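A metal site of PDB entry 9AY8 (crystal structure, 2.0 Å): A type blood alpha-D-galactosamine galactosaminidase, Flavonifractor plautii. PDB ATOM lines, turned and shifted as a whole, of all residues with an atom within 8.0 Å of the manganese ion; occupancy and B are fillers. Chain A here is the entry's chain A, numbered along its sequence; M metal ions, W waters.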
ATOM      1  N   ASP A 146     -21.927  -7.262   8.943  1.00  0.00           N
ATOM      2  CA  ASP A 146     -20.962  -6.198   9.073  1.00  0.00           C
ATOM      3  C   ASP A 146     -19.557  -6.709   8.749  1.00  0.00           C
ATOM      4  O   ASP A 146     -18.691  -5.913   8.395  1.00  0.00           O
ATOM      5  CB  ASP A 146     -21.080  -5.521  10.421  1.00  0.00           C
ATOM      6  CG  ASP A 146     -20.820  -6.430  11.616  1.00  0.00           C
ATOM      7  OD1 ASP A 146     -21.213  -7.587  11.551  1.00  0.00           O
ATOM      8  OD2 ASP A 146     -20.224  -5.953  12.600  1.00  0.00           O
ATOM      9  N   LYS A 167     -10.005 -10.403   8.241  1.00  0.00           N
ATOM     10  CA  LYS A 167     -11.357  -9.904   8.383  1.00  0.00           C
ATOM     11  C   LYS A 167     -11.688  -9.052   7.174  1.00  0.00           C
ATOM     12  O   LYS A 167     -10.936  -8.133   6.821  1.00  0.00           O
ATOM     13  CB  LYS A 167     -11.539  -9.065   9.646  1.00  0.00           C
ATOM     14  CG  LYS A 167     -12.984  -8.679   9.913  1.00  0.00           C
ATOM     15  CD  LYS A 167     -13.196  -8.031  11.282  1.00  0.00           C
ATOM     16  CE  LYS A 167     -12.537  -6.711  11.385  1.00  0.00           C
ATOM     17  NZ  LYS A 167     -12.916  -6.048  12.628  1.00  0.00           N
ATOM     18  N   ILE A 168     -12.823  -9.365   6.563  1.00  0.00           N
ATOM     19  CA  ILE A 168     -13.388  -8.576   5.491  1.00  0.00           C
ATOM     20  C   ILE A 168     -14.452  -7.715   6.137  1.00  0.00           C
ATOM     21  O   ILE A 168     -15.554  -8.160   6.456  1.00  0.00           O
ATOM     22  CB  ILE A 168     -13.955  -9.446   4.367  1.00  0.00           C
ATOM     23  CG1 ILE A 168     -12.897 -10.409   3.841  1.00  0.00           C
ATOM     24  CG2 ILE A 168     -14.527  -8.575   3.261  1.00  0.00           C
ATOM     25  CD1 ILE A 168     -13.388 -11.445   2.855  1.00  0.00           C
ATOM     26  N   ASP A 169     -14.078  -6.455   6.348  1.00  0.00           N
ATOM     27  CA  ASP A 169     -14.952  -5.491   6.954  1.00  0.00           C
ATOM     28  C   ASP A 169     -15.872  -4.946   5.853  1.00  0.00           C
ATOM     29  O   ASP A 169     -15.397  -4.451   4.848  1.00  0.00           O
ATOM     30  CB  ASP A 169     -14.130  -4.427   7.623  1.00  0.00           C
ATOM     31  CG  ASP A 169     -14.889  -3.392   8.440  1.00  0.00           C
ATOM     32  OD1 ASP A 169     -16.115  -3.243   8.258  1.00  0.00           O
ATOM     33  OD2 ASP A 169     -14.223  -2.748   9.245  1.00  0.00           O
ATOM     34  N   LEU A 170     -17.193  -5.026   6.090  1.00  0.00           N
ATOM     35  CA  LEU A 170     -18.161  -4.550   5.121  1.00  0.00           C
ATOM     36  C   LEU A 170     -18.661  -3.147   5.463  1.00  0.00           C
ATOM     37  O   LEU A 170     -19.551  -2.652   4.769  1.00  0.00           O
ATOM     38  CB  LEU A 170     -19.309  -5.563   5.080  1.00  0.00           C
ATOM     39  CG  LEU A 170     -18.911  -7.006   4.807  1.00  0.00           C
ATOM     40  CD1 LEU A 170     -20.064  -7.980   4.930  1.00  0.00           C
ATOM     41  CD2 LEU A 170     -18.307  -7.113   3.440  1.00  0.00           C
ATOM     42  N   THR A 171     -18.111  -2.510   6.508  1.00  0.00           N
ATOM     43  CA  THR A 171     -18.577  -1.183   6.940  1.00  0.00           C
ATOM     44  C   THR A 171     -17.532  -0.108   6.617  1.00  0.00           C
ATOM     45  O   THR A 171     -17.780   1.069   6.839  1.00  0.00           O
ATOM     46  CB  THR A 171     -18.878  -1.170   8.446  1.00  0.00           C
ATOM     47  OG1 THR A 171     -17.629  -1.375   9.117  1.00  0.00           O
ATOM     48  CG2 THR A 171     -19.812  -2.296   8.867  1.00  0.00           C
ATOM     49  N   ASP A 172     -16.358  -0.495   6.132  1.00  0.00           N
ATOM     50  CA  ASP A 172     -15.251   0.447   5.984  1.00  0.00           C
ATOM     51  C   ASP A 172     -15.249   0.964   4.538  1.00  0.00           C
ATOM     52  O   ASP A 172     -16.204   0.773   3.807  1.00  0.00           O
ATOM     53  CB  ASP A 172     -13.917  -0.168   6.373  1.00  0.00           C
ATOM     54  CG  ASP A 172     -13.475  -1.293   5.455  1.00  0.00           C
ATOM     55  OD1 ASP A 172     -14.330  -1.644   4.629  1.00  0.00           O
ATOM     56  OD2 ASP A 172     -12.320  -1.831   5.565  1.00  0.00           O
ATOM     57  N   SER A 173     -14.164   1.621   4.122  1.00  0.00           N
ATOM     58  CA  SER A 173     -14.067   2.125   2.771  1.00  0.00           C
ATOM     59  C   SER A 173     -13.408   1.103   1.838  1.00  0.00           C
ATOM     60  O   SER A 173     -13.725   1.024   0.680  1.00  0.00           O
ATOM     61  CB  SER A 173     -13.357   3.465   2.771  1.00  0.00           C
ATOM     62  OG  SER A 173     -12.686   3.708   1.560  1.00  0.00           O
ATOM     63  N   GLY A 174     -12.497   0.287   2.333  1.00  0.00           N
ATOM     64  CA  GLY A 174     -11.732  -0.590   1.471  1.00  0.00           C
ATOM     65  C   GLY A 174     -12.537  -1.776   0.911  1.00  0.00           C
ATOM     66  O   GLY A 174     -13.643  -2.099   1.372  1.00  0.00           O
ATOM     67  N   LYS A 175     -11.969  -2.411  -0.110  1.00  0.00           N
ATOM     68  CA  LYS A 175     -12.547  -3.599  -0.709  1.00  0.00           C
ATOM     69  C   LYS A 175     -11.478  -4.677  -0.689  1.00  0.00           C
ATOM     70  O   LYS A 175     -10.518  -4.589  -1.426  1.00  0.00           O
ATOM     71  CB  LYS A 175     -13.000  -3.395  -2.153  1.00  0.00           C
ATOM     72  CG  LYS A 175     -14.193  -2.505  -2.320  1.00  0.00           C
ATOM     73  CD  LYS A 175     -15.511  -3.095  -1.788  1.00  0.00           C
ATOM     74  CE  LYS A 175     -16.526  -1.974  -1.831  1.00  0.00           C
ATOM     75  NZ  LYS A 175     -17.877  -2.486  -1.826  1.00  0.00           N
ATOM     76  N   PHE A 176     -11.666  -5.670   0.158  1.00  0.00           N
ATOM     77  CA  PHE A 176     -10.703  -6.729   0.291  1.00  0.00           C
ATOM     78  C   PHE A 176     -10.625  -7.513  -1.016  1.00  0.00           C
ATOM     79  O   PHE A 176     -11.662  -7.862  -1.590  1.00  0.00           O
ATOM     80  CB  PHE A 176     -11.131  -7.664   1.427  1.00  0.00           C
ATOM     81  CG  PHE A 176     -10.095  -8.752   1.679  1.00  0.00           C
ATOM     82  CD1 PHE A 176     -10.112  -9.942   0.977  1.00  0.00           C
ATOM     83  CD2 PHE A 176      -9.103  -8.543   2.628  1.00  0.00           C
ATOM     84  CE1 PHE A 176      -9.160 -10.924   1.231  1.00  0.00           C
ATOM     85  CE2 PHE A 176      -8.156  -9.517   2.883  1.00  0.00           C
ATOM     86  CZ  PHE A 176      -8.171 -10.704   2.172  1.00  0.00           C
ATOM     87  N   GLU A 219     -14.130  -9.142  -1.708  1.00  0.00           N
ATOM     88  CA  GLU A 219     -15.254  -8.425  -1.137  1.00  0.00           C
ATOM     89  C   GLU A 219     -16.163  -7.983  -2.271  1.00  0.00           C
ATOM     90  O   GLU A 219     -15.672  -7.555  -3.300  1.00  0.00           O
ATOM     91  CB  GLU A 219     -14.744  -7.239  -0.320  1.00  0.00           C
ATOM     92  CG  GLU A 219     -15.876  -6.531   0.425  1.00  0.00           C
ATOM     93  CD  GLU A 219     -15.347  -5.443   1.346  1.00  0.00           C
ATOM     94  OE1 GLU A 219     -16.192  -4.662   1.778  1.00  0.00           O
ATOM     95  OE2 GLU A 219     -14.117  -5.406   1.656  1.00  0.00           O
ATOM     96  N   THR A 220     -17.472  -8.075  -2.056  1.00  0.00           N
ATOM     97  CA  THR A 220     -18.483  -7.657  -3.014  1.00  0.00           C
ATOM     98  C   THR A 220     -19.201  -6.463  -2.423  1.00  0.00           C
ATOM     99  O   THR A 220     -18.814  -5.929  -1.396  1.00  0.00           O
ATOM    100  CB  THR A 220     -19.413  -8.840  -3.281  1.00  0.00           C
ATOM    101  OG1 THR A 220     -20.194  -9.130  -2.128  1.00  0.00           O
ATOM    102  CG2 THR A 220     -18.634 -10.106  -3.588  1.00  0.00           C
ATOM    103  N   SER A 221     -20.329  -6.077  -3.053  1.00  0.00           N
ATOM    104  CA  SER A 221     -20.999  -4.864  -2.638  1.00  0.00           C
ATOM    105  C   SER A 221     -21.475  -4.977  -1.189  1.00  0.00           C
ATOM    106  O   SER A 221     -21.482  -3.981  -0.485  1.00  0.00           O
ATOM    107  CB  SER A 221     -22.123  -4.507  -3.576  1.00  0.00           C
ATOM    108  OG  SER A 221     -23.023  -5.606  -3.631  1.00  0.00           O
ATOM    109  N   SER A 223     -20.990  -8.273   0.605  1.00  0.00           N
ATOM    110  CA  SER A 223     -20.576  -9.568   1.087  1.00  0.00           C
ATOM    111  C   SER A 223     -19.177  -9.857   0.565  1.00  0.00           C
ATOM    112  O   SER A 223     -18.443  -8.919   0.246  1.00  0.00           O
ATOM    113  CB  SER A 223     -21.599 -10.640   0.676  1.00  0.00           C
ATOM    114  OG  SER A 223     -21.373 -11.885   1.308  1.00  0.00           O
HETATM  115 MN    MN M   1     -14.578  -3.323   3.048  1.00  0.00          MN
HETATM  116  O   HOH W   1     -16.657  -1.829   2.797  1.00  0.00           O
HETATM  117  O   HOH W   2     -12.124  -3.739   3.790  1.00  0.00           O
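The manganese ion is bound by the backbone carbonyl oxygen (O) of Gly 174 (2.3 Å), the backbone carbonyl oxygen (O) of Asp 169 (2.3 Å), the side-chain carboxylate (OD1) of Asp 172 (2.3 Å), the side-chain carboxylate (OE1) of Glu 219 (2.5 Å), the side-chain carboxylate (OE2) of Glu 219 (2.5 Å), water W1 (2.6 Å) and water W2 (2.6 Å).
The manganese ion has seven donor atoms within binding distance.
Within 4 Å of the manganese ion: Asp 169, Asp 172, Gly 174 and Glu 219.
Along chain A the residues within 4 Å of the manganese ion span positions 169 to 219.
OG1 of Thr 171 sits at hydrogen-bond distance from OD1 of Asp 169, 2.6 Å away.
The backbone NH of Glu 219 is in hydrogen-bond range of the backbone carbonyl oxygen of Phe 176 (2.8 Å).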
